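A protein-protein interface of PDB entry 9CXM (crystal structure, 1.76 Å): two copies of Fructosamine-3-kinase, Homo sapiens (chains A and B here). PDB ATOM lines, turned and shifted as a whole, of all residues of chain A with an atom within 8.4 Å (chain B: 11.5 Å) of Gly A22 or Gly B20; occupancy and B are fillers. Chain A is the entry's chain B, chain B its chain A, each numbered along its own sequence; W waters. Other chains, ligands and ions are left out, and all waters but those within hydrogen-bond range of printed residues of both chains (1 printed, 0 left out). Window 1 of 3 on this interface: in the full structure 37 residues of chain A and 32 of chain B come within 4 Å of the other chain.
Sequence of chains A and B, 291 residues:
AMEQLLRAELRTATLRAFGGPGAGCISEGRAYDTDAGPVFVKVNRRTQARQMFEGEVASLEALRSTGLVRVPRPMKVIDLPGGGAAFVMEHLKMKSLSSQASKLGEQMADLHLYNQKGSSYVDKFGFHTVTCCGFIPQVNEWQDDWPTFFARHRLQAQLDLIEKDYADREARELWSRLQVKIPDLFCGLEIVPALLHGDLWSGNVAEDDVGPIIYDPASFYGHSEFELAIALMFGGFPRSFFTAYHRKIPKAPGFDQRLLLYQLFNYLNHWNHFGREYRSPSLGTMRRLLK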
ATOM      1  N   GLY A  19     -39.440  -4.009  -9.491  1.00  0.00           N
ATOM      2  CA  GLY A  19     -38.474  -4.593 -10.395  1.00  0.00           C
ATOM      3  C   GLY A  19     -38.987  -5.919 -10.930  1.00  0.00           C
ATOM      4  O   GLY A  19     -38.256  -6.660 -11.593  1.00  0.00           O
ATOM      5  N   GLY A  22     -30.414  -5.390 -16.712  1.00  0.00           N
ATOM      6  CA  GLY A  22     -30.640  -6.824 -16.827  1.00  0.00           C
ATOM      7  C   GLY A  22     -31.604  -7.348 -15.772  1.00  0.00           C
ATOM      8  O   GLY A  22     -31.816  -6.678 -14.758  1.00  0.00           O
ATOM      9  N   ALA A  23     -32.183  -8.537 -16.004  1.00  0.00           N
ATOM     10  CA  ALA A  23     -33.147  -9.156 -15.088  1.00  0.00           C
ATOM     11  C   ALA A  23     -33.523 -10.553 -15.581  1.00  0.00           C
ATOM     12  O   ALA A  23     -33.578 -10.766 -16.797  1.00  0.00           O
ATOM     13  CB  ALA A  23     -34.404  -8.292 -14.949  1.00  0.00           C
ATOM     14  N   GLY A  24     -33.795 -11.489 -14.663  1.00  0.00           N
ATOM     15  CA  GLY A  24     -34.120 -12.893 -14.886  1.00  0.00           C
ATOM     16  C   GLY A  24     -32.983 -13.815 -14.431  1.00  0.00           C
ATOM     17  O   GLY A  24     -31.811 -13.416 -14.387  1.00  0.00           O
ATOM     18  N   CYS A  25     -33.327 -15.079 -14.105  1.00  0.00           N
ATOM     19  CA  CYS A  25     -32.287 -16.019 -13.659  1.00  0.00           C
ATOM     20  C   CYS A  25     -31.745 -16.889 -14.782  1.00  0.00           C
ATOM     21  O   CYS A  25     -30.824 -17.681 -14.550  1.00  0.00           O
ATOM     22  CB  CYS A  25     -32.766 -16.946 -12.526  1.00  0.00           C
ATOM     23  SG  CYS A  25     -33.398 -16.233 -11.022  1.00  0.00           S
ATOM     24  N   SER A  27     -31.799 -15.682 -18.548  1.00  0.00           N
ATOM     25  CA  SER A  27     -31.301 -14.879 -19.647  1.00  0.00           C
ATOM     26  C   SER A  27     -31.066 -13.462 -19.143  1.00  0.00           C
ATOM     27  O   SER A  27     -31.573 -13.065 -18.094  1.00  0.00           O
ATOM     28  CB  SER A  27     -32.323 -14.833 -20.804  1.00  0.00           C
ATOM     29  OG  SER A  27     -32.637 -16.144 -21.257  1.00  0.00           O
ATOM     30  N   GLU A  28     -30.331 -12.696 -19.929  1.00  0.00           N
ATOM     31  CA  GLU A  28     -30.163 -11.266 -19.669  1.00  0.00           C
ATOM     32  C   GLU A  28     -31.290 -10.533 -20.404  1.00  0.00           C
ATOM     33  O   GLU A  28     -31.455 -10.735 -21.606  1.00  0.00           O
ATOM     34  CB  GLU A  28     -28.792 -10.829 -20.173  1.00  0.00           C
ATOM     35  CG  GLU A  28     -28.511  -9.353 -20.047  1.00  0.00           C
ATOM     36  CD  GLU A  28     -27.060  -9.041 -20.376  1.00  0.00           C
ATOM     37  OE1 GLU A  28     -26.319  -9.995 -20.729  1.00  0.00           O
ATOM     38  OE2 GLU A  28     -26.673  -7.852 -20.267  1.00  0.00           O
ATOM     39  N   GLY A  29     -32.096  -9.764 -19.676  1.00  0.00           N
ATOM     40  CA  GLY A  29     -33.251  -9.053 -20.227  1.00  0.00           C
ATOM     41  C   GLY A  29     -33.087  -7.537 -20.229  1.00  0.00           C
ATOM     42  O   GLY A  29     -32.707  -6.952 -19.217  1.00  0.00           O
ATOM     43  N   ARG A  30     -33.382  -6.906 -21.379  1.00  0.00           N
ATOM     44  CA  ARG A  30     -33.222  -5.456 -21.525  1.00  0.00           C
ATOM     45  C   ARG A  30     -34.320  -4.846 -22.384  1.00  0.00           C
ATOM     46  O   ARG A  30     -34.687  -5.427 -23.392  1.00  0.00           O
ATOM     47  CB  ARG A  30     -31.869  -5.118 -22.158  1.00  0.00           C
ATOM     48  CG  ARG A  30     -30.669  -5.553 -21.343  1.00  0.00           C
ATOM     49  CD  ARG A  30     -29.456  -4.729 -21.770  1.00  0.00           C
ATOM     50  NE  ARG A  30     -28.197  -5.226 -21.223  1.00  0.00           N
ATOM     51  CZ  ARG A  30     -27.105  -4.478 -21.121  1.00  0.00           C
ATOM     52  NH1 ARG A  30     -27.111  -3.203 -21.483  1.00  0.00           N
ATOM     53  NH2 ARG A  30     -25.987  -5.018 -20.635  1.00  0.00           N
ATOM     54  N   ALA A  31     -34.833  -3.676 -21.999  1.00  0.00           N
ATOM     55  CA  ALA A  31     -35.822  -2.958 -22.800  1.00  0.00           C
ATOM     56  C   ALA A  31     -35.158  -1.862 -23.634  1.00  0.00           C
ATOM     57  O   ALA A  31     -34.254  -1.159 -23.153  1.00  0.00           O
ATOM     58  CB  ALA A  31     -36.881  -2.315 -21.930  1.00  0.00           C
ATOM     59  N   TYR A  32     -35.623  -1.726 -24.876  1.00  0.00           N
ATOM     60  CA  TYR A  32     -35.107  -0.736 -25.814  1.00  0.00           C
ATOM     61  C   TYR A  32     -36.255  -0.002 -26.478  1.00  0.00           C
ATOM     62  O   TYR A  32     -37.249  -0.616 -26.901  1.00  0.00           O
ATOM     63  CB  TYR A  32     -34.274  -1.365 -26.932  1.00  0.00           C
ATOM     64  CG  TYR A  32     -33.043  -2.052 -26.474  1.00  0.00           C
ATOM     65  CD1 TYR A  32     -31.871  -1.335 -26.216  1.00  0.00           C
ATOM     66  CD2 TYR A  32     -33.027  -3.437 -26.332  1.00  0.00           C
ATOM     67  CE1 TYR A  32     -30.713  -1.988 -25.806  1.00  0.00           C
ATOM     68  CE2 TYR A  32     -31.883  -4.089 -25.938  1.00  0.00           C
ATOM     69  CZ  TYR A  32     -30.725  -3.357 -25.685  1.00  0.00           C
ATOM     70  OH  TYR A  32     -29.624  -4.013 -25.274  1.00  0.00           O
ATOM     71  N   PHE A  40     -38.662  -5.710 -25.741  1.00  0.00           N
ATOM     72  CA  PHE A  40     -37.928  -6.344 -24.661  1.00  0.00           C
ATOM     73  C   PHE A  40     -37.105  -7.459 -25.266  1.00  0.00           C
ATOM     74  O   PHE A  40     -37.597  -8.189 -26.118  1.00  0.00           O
ATOM     75  CB  PHE A  40     -38.888  -6.886 -23.578  1.00  0.00           C
ATOM     76  CG  PHE A  40     -38.185  -7.412 -22.414  1.00  0.00           C
ATOM     77  CD1 PHE A  40     -37.625  -6.537 -21.496  1.00  0.00           C
ATOM     78  CD2 PHE A  40     -38.070  -8.791 -22.207  1.00  0.00           C
ATOM     79  CE1 PHE A  40     -36.932  -7.018 -20.398  1.00  0.00           C
ATOM     80  CE2 PHE A  40     -37.380  -9.282 -21.085  1.00  0.00           C
ATOM     81  CZ  PHE A  40     -36.813  -8.363 -20.192  1.00  0.00           C
ATOM     82  N   VAL A  41     -35.820  -7.551 -24.893  1.00  0.00           N
ATOM     83  CA  VAL A  41     -34.898  -8.462 -25.541  1.00  0.00           C
ATOM     84  C   VAL A  41     -34.264  -9.337 -24.463  1.00  0.00           C
ATOM     85  O   VAL A  41     -33.767  -8.809 -23.468  1.00  0.00           O
ATOM     86  CB  VAL A  41     -33.784  -7.716 -26.310  1.00  0.00           C
ATOM     87  CG1 VAL A  41     -32.965  -8.717 -27.031  1.00  0.00           C
ATOM     88  CG2 VAL A  41     -34.396  -6.779 -27.354  1.00  0.00           C
ATOM     89  N   ARG B  16     -32.650   2.727 -27.820  1.00  0.00           N
ATOM     90  CA  ARG B  16     -32.203   3.397 -26.607  1.00  0.00           C
ATOM     91  C   ARG B  16     -32.672   2.574 -25.431  1.00  0.00           C
ATOM     92  O   ARG B  16     -33.879   2.387 -25.246  1.00  0.00           O
ATOM     93  CB  ARG B  16     -32.733   4.832 -26.511  1.00  0.00           C
ATOM     94  N   ALA B  17     -31.721   2.075 -24.666  1.00  0.00           N
ATOM     95  CA  ALA B  17     -32.037   1.292 -23.484  1.00  0.00           C
ATOM     96  C   ALA B  17     -32.797   2.133 -22.468  1.00  0.00           C
ATOM     97  O   ALA B  17     -32.637   3.354 -22.400  1.00  0.00           O
ATOM     98  CB  ALA B  17     -30.752   0.727 -22.878  1.00  0.00           C
ATOM     99  N   PHE B  18     -33.746   1.502 -21.786  1.00  0.00           N
ATOM    100  CA  PHE B  18     -34.469   2.143 -20.698  1.00  0.00           C
ATOM    101  C   PHE B  18     -34.865   1.068 -19.693  1.00  0.00           C
ATOM    102  O   PHE B  18     -34.731  -0.130 -19.958  1.00  0.00           O
ATOM    103  CB  PHE B  18     -35.658   2.946 -21.209  1.00  0.00           C
ATOM    104  CG  PHE B  18     -36.790   2.105 -21.718  1.00  0.00           C
ATOM    105  CD1 PHE B  18     -36.810   1.681 -23.039  1.00  0.00           C
ATOM    106  CD2 PHE B  18     -37.858   1.778 -20.884  1.00  0.00           C
ATOM    107  CE1 PHE B  18     -37.878   0.921 -23.518  1.00  0.00           C
ATOM    108  CE2 PHE B  18     -38.924   1.042 -21.357  1.00  0.00           C
ATOM    109  CZ  PHE B  18     -38.933   0.610 -22.667  1.00  0.00           C
ATOM    110  N   GLY B  19     -35.253   1.499 -18.497  1.00  0.00           N
ATOM    111  CA  GLY B  19     -35.722   0.557 -17.496  1.00  0.00           C
ATOM    112  C   GLY B  19     -34.657  -0.283 -16.821  1.00  0.00           C
ATOM    113  O   GLY B  19     -35.007  -1.179 -16.038  1.00  0.00           O
ATOM    114  N   GLY B  20     -33.379  -0.047 -17.111  1.00  0.00           N
ATOM    115  CA  GLY B  20     -32.296  -0.780 -16.472  1.00  0.00           C
ATOM    116  C   GLY B  20     -32.285  -2.276 -16.725  1.00  0.00           C
ATOM    117  O   GLY B  20     -31.391  -2.989 -16.250  1.00  0.00           O
ATOM    118  N   GLY B  29     -34.736 -13.249  -4.231  1.00  0.00           N
ATOM    119  CA  GLY B  29     -34.468 -11.937  -3.692  1.00  0.00           C
ATOM    120  C   GLY B  29     -35.439 -10.962  -4.323  1.00  0.00           C
ATOM    121  O   GLY B  29     -35.559 -10.887  -5.549  1.00  0.00           O
ATOM    122  N   ALA B  31     -37.113  -6.924  -4.070  1.00  0.00           N
ATOM    123  CA  ALA B  31     -37.013  -5.563  -3.527  1.00  0.00           C
ATOM    124  C   ALA B  31     -38.423  -5.149  -3.146  1.00  0.00           C
ATOM    125  O   ALA B  31     -39.371  -5.630  -3.788  1.00  0.00           O
ATOM    126  CB  ALA B  31     -36.448  -4.636  -4.565  1.00  0.00           C
ATOM    127  N   PHE B  40     -34.089  -4.178   0.246  1.00  0.00           N
ATOM    128  CA  PHE B  40     -33.947  -5.388  -0.532  1.00  0.00           C
ATOM    129  C   PHE B  40     -33.920  -6.560   0.430  1.00  0.00           C
ATOM    130  O   PHE B  40     -33.230  -6.513   1.456  1.00  0.00           O
ATOM    131  CB  PHE B  40     -32.676  -5.342  -1.405  1.00  0.00           C
ATOM    132  CG  PHE B  40     -32.556  -6.476  -2.331  1.00  0.00           C
ATOM    133  CD1 PHE B  40     -33.231  -6.473  -3.549  1.00  0.00           C
ATOM    134  CD2 PHE B  40     -31.788  -7.577  -2.006  1.00  0.00           C
ATOM    135  CE1 PHE B  40     -33.125  -7.563  -4.414  1.00  0.00           C
ATOM    136  CE2 PHE B  40     -31.671  -8.638  -2.853  1.00  0.00           C
ATOM    137  CZ  PHE B  40     -32.331  -8.651  -4.055  1.00  0.00           C
ATOM    138  N   HIS B  91     -31.593  -0.890   0.259  1.00  0.00           N
ATOM    139  CA  HIS B  91     -31.683  -1.071  -1.179  1.00  0.00           C
ATOM    140  C   HIS B  91     -30.759  -0.084  -1.884  1.00  0.00           C
ATOM    141  O   HIS B  91     -30.648   1.074  -1.472  1.00  0.00           O
ATOM    142  CB  HIS B  91     -33.124  -0.854  -1.661  1.00  0.00           C
ATOM    143  CG  HIS B  91     -33.293  -1.032  -3.136  1.00  0.00           C
ATOM    144  ND1 HIS B  91     -33.107   0.000  -4.031  1.00  0.00           N
ATOM    145  CD2 HIS B  91     -33.565  -2.131  -3.875  1.00  0.00           C
ATOM    146  CE1 HIS B  91     -33.303  -0.454  -5.260  1.00  0.00           C
ATOM    147  NE2 HIS B  91     -33.582  -1.742  -5.193  1.00  0.00           N
ATOM    148  N   LEU B  92     -30.104  -0.576  -2.923  1.00  0.00           N
ATOM    149  CA  LEU B  92     -29.192   0.278  -3.720  1.00  0.00           C
ATOM    150  C   LEU B  92     -29.533   0.127  -5.207  1.00  0.00           C
ATOM    151  O   LEU B  92     -29.634  -1.003  -5.675  1.00  0.00           O
ATOM    152  CB  LEU B  92     -27.744  -0.131  -3.425  1.00  0.00           C
ATOM    153  CG  LEU B  92     -27.245   0.128  -2.008  1.00  0.00           C
ATOM    154  CD1 LEU B  92     -25.919  -0.574  -1.776  1.00  0.00           C
ATOM    155  CD2 LEU B  92     -27.110   1.618  -1.743  1.00  0.00           C
ATOM    156  N   LYS B  93     -29.734   1.252  -5.893  1.00  0.00           N
ATOM    157  CA  LYS B  93     -29.978   1.230  -7.352  1.00  0.00           C
ATOM    158  C   LYS B  93     -28.624   0.935  -7.976  1.00  0.00           C
ATOM    159  O   LYS B  93     -27.710   1.722  -7.755  1.00  0.00           O
ATOM    160  CB  LYS B  93     -30.561   2.565  -7.812  1.00  0.00           C
ATOM    161  N   MET B  94     -28.517  -0.176  -8.686  1.00  0.00           N
ATOM    162  CA  MET B  94     -27.183  -0.588  -9.163  1.00  0.00           C
ATOM    163  C   MET B  94     -27.193  -0.930 -10.650  1.00  0.00           C
ATOM    164  O   MET B  94     -28.244  -1.322 -11.168  1.00  0.00           O
ATOM    165  CB  MET B  94     -26.744  -1.829  -8.384  1.00  0.00           C
ATOM    166  CG  MET B  94     -26.619  -1.618  -6.902  1.00  0.00           C
ATOM    167  SD  MET B  94     -26.069  -3.147  -6.120  1.00  0.00           S
ATOM    168  CE  MET B  94     -27.255  -4.309  -6.789  1.00  0.00           C
ATOM    169  N   LYS B  95     -26.044  -0.790 -11.291  1.00  0.00           N
ATOM    170  CA  LYS B  95     -25.895  -1.168 -12.707  1.00  0.00           C
ATOM    171  C   LYS B  95     -24.586  -1.942 -12.797  1.00  0.00           C
ATOM    172  O   LYS B  95     -23.808  -1.887 -11.841  1.00  0.00           O
ATOM    173  CB  LYS B  95     -25.862   0.082 -13.589  1.00  0.00           C
ATOM    174  CG  LYS B  95     -24.477   0.645 -13.867  1.00  0.00           C
ATOM    175  CD  LYS B  95     -24.480   1.889 -14.729  1.00  0.00           C
ATOM    176  CE  LYS B  95     -24.923   3.129 -13.985  1.00  0.00           C
ATOM    177  NZ  LYS B  95     -24.571   4.362 -14.726  1.00  0.00           N
ATOM    178  N   SER B  96     -24.368  -2.628 -13.910  1.00  0.00           N
ATOM    179  CA  SER B  96     -23.135  -3.422 -14.101  1.00  0.00           C
ATOM    180  C   SER B  96     -21.912  -2.532 -13.889  1.00  0.00           C
ATOM    181  O   SER B  96     -21.978  -1.353 -14.222  1.00  0.00           O
ATOM    182  CB  SER B  96     -23.110  -4.070 -15.465  1.00  0.00           C
ATOM    183  OG  SER B  96     -24.032  -5.144 -15.528  1.00  0.00           O
ATOM    184  N   LEU B  97     -20.851  -3.112 -13.337  1.00  0.00           N
ATOM    185  CA  LEU B  97     -19.594  -2.352 -13.146  1.00  0.00           C
ATOM    186  C   LEU B  97     -18.999  -2.048 -14.514  1.00  0.00           C
ATOM    187  O   LEU B  97     -18.747  -2.989 -15.264  1.00  0.00           O
ATOM    188  CB  LEU B  97     -18.599  -3.160 -12.312  1.00  0.00           C
ATOM    189  CG  LEU B  97     -17.276  -2.458 -12.015  1.00  0.00           C
ATOM    190  CD1 LEU B  97     -17.489  -1.259 -11.109  1.00  0.00           C
ATOM    191  CD2 LEU B  97     -16.283  -3.427 -11.396  1.00  0.00           C
ATOM    192  N   GLY B 203     -20.569 -11.011 -10.754  1.00  0.00           N
ATOM    193  CA  GLY B 203     -21.974 -10.883 -10.383  1.00  0.00           C
ATOM    194  C   GLY B 203     -22.201 -10.300  -9.010  1.00  0.00           C
ATOM    195  O   GLY B 203     -23.343 -10.048  -8.636  1.00  0.00           O
ATOM    196  N   VAL B 205     -20.527  -7.461  -7.959  1.00  0.00           N
ATOM    197  CA  VAL B 205     -20.057  -6.081  -7.958  1.00  0.00           C
ATOM    198  C   VAL B 205     -20.926  -5.280  -8.921  1.00  0.00           C
ATOM    199  O   VAL B 205     -21.491  -5.825  -9.876  1.00  0.00           O
ATOM    200  CB  VAL B 205     -18.564  -5.963  -8.371  1.00  0.00           C
ATOM    201  CG1 VAL B 205     -17.732  -6.808  -7.383  1.00  0.00           C
ATOM    202  CG2 VAL B 205     -18.351  -6.444  -9.848  1.00  0.00           C
ATOM    203  N   ALA B 206     -20.979  -3.977  -8.693  1.00  0.00           N
ATOM    204  CA  ALA B 206     -21.871  -3.128  -9.474  1.00  0.00           C
ATOM    205  C   ALA B 206     -21.451  -1.685  -9.284  1.00  0.00           C
ATOM    206  O   ALA B 206     -20.403  -1.386  -8.696  1.00  0.00           O
ATOM    207  CB  ALA B 206     -23.326  -3.358  -9.037  1.00  0.00           C
ATOM    208  N   GLU B 207     -22.322  -0.775  -9.704  1.00  0.00           N
ATOM    209  CA  GLU B 207     -22.011   0.648  -9.456  1.00  0.00           C
ATOM    210  C   GLU B 207     -23.262   1.515  -9.564  1.00  0.00           C
ATOM    211  O   GLU B 207     -24.264   1.044 -10.119  1.00  0.00           O
ATOM    212  CB  GLU B 207     -20.976   1.150 -10.460  1.00  0.00           C
ATOM    213  CG  GLU B 207     -21.510   1.277 -11.874  1.00  0.00           C
ATOM    214  CD  GLU B 207     -20.475   1.716 -12.895  1.00  0.00           C
ATOM    215  OE1 GLU B 207     -19.369   1.152 -12.891  1.00  0.00           O
ATOM    216  OE2 GLU B 207     -20.778   2.633 -13.678  1.00  0.00           O
ATOM    217  N   ASP B 209     -24.300   6.115  -9.645  1.00  0.00           N
ATOM    218  CA  ASP B 209     -23.760   7.373 -10.221  1.00  0.00           C
ATOM    219  C   ASP B 209     -22.655   7.921  -9.310  1.00  0.00           C
ATOM    220  O   ASP B 209     -21.895   8.788  -9.773  1.00  0.00           O
ATOM    221  CB  ASP B 209     -24.870   8.403 -10.448  1.00  0.00           C
ATOM    222  CG  ASP B 209     -25.796   8.062 -11.601  1.00  0.00           C
ATOM    223  OD1 ASP B 209     -26.788   8.791 -11.787  1.00  0.00           O
ATOM    224  OD2 ASP B 209     -25.514   7.074 -12.304  1.00  0.00           O
ATOM    225  N   TYR B 215     -21.125  -6.601  -2.893  1.00  0.00           N
ATOM    226  CA  TYR B 215     -22.145  -7.200  -2.023  1.00  0.00           C
ATOM    227  C   TYR B 215     -21.980  -8.721  -2.045  1.00  0.00           C
ATOM    228  O   TYR B 215     -21.090  -9.266  -2.711  1.00  0.00           O
ATOM    229  CB  TYR B 215     -23.586  -6.751  -2.472  1.00  0.00           C
ATOM    230  CG  TYR B 215     -23.820  -6.969  -3.963  1.00  0.00           C
ATOM    231  CD1 TYR B 215     -24.270  -8.185  -4.444  1.00  0.00           C
ATOM    232  CD2 TYR B 215     -23.634  -5.927  -4.864  1.00  0.00           C
ATOM    233  CE1 TYR B 215     -24.456  -8.387  -5.793  1.00  0.00           C
ATOM    234  CE2 TYR B 215     -23.820  -6.117  -6.204  1.00  0.00           C
ATOM    235  CZ  TYR B 215     -24.233  -7.335  -6.660  1.00  0.00           C
ATOM    236  OH  TYR B 215     -24.427  -7.520  -7.992  1.00  0.00           O
HETATM  237  O   HOH W   1     -33.931  -2.642 -19.406  1.00  0.00           O
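N of Phe B18 lies within hydrogen-bond range of O of Ala A31 (3.0 Å).
O of Gly B20 sits at hydrogen-bond distance from N of Gly A22, at 2.6 Å.
Among the printed residues, merely in contact across the chains: Ala A31 with Ala B17 (3.3 Å), Tyr A32 with Arg B16 (3.4 Å), Tyr A32 with Phe B18 (3.5 Å) and Tyr A32 with Ala B17 (3.7 Å).
Gly A22 touches just one residue of chain B: Gly B20 (2.6 Å).
No residue of chain B comes within 4 Å of Ala A23.
No residue of chain B comes within 4 Å of Gly A24.
Glu A28 touches none of the printed residues of chain B.
No residue of chain B comes within 4 Å of Gly A29.
Of chain B, only Ala B17 (3.3 Å) and Phe B18 (3.0 Å) come within 4 Å of Ala A31.
Of the printed residues of chain B, Tyr A32 touches Arg B16 (3.4 Å), Ala B17 (3.7 Å) and Phe B18 (3.5 Å).
Of the printed residues of chain A, Phe B18 touches Ala A31 (3.0 Å) and Tyr A32 (3.5 Å).
No residue of chain A comes within 4 Å of Gly B19.
Gly B20 touches just one residue of chain A: Gly A22 (2.6 Å).
The nearest residue of chain A that does not touch Gly B20 is Gly A29 (5.1 Å).
Hydrophobic or aromatic side chains of chain B within 4 Å of the printed part of chain A: Ala B17 and Phe B18.
Printed residues of chain A that touch a printed residue of chain B: Gly A22, Ala A31 and Tyr A32.
Among the printed residues, 6 pairs touch across the chains.
Positions printed for both chains: 19, 29, 31 and 40.
Of the 6 pairs that touch across the chains among the printed residues, none has its exchanged pair printed and touching as well.
Water W1 lies within hydrogen-bond range of the backbone carbonyl oxygen (O) of Phe B18 (2.7 Å) and the backbone NH (N) of Ala A31 (2.9 Å).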
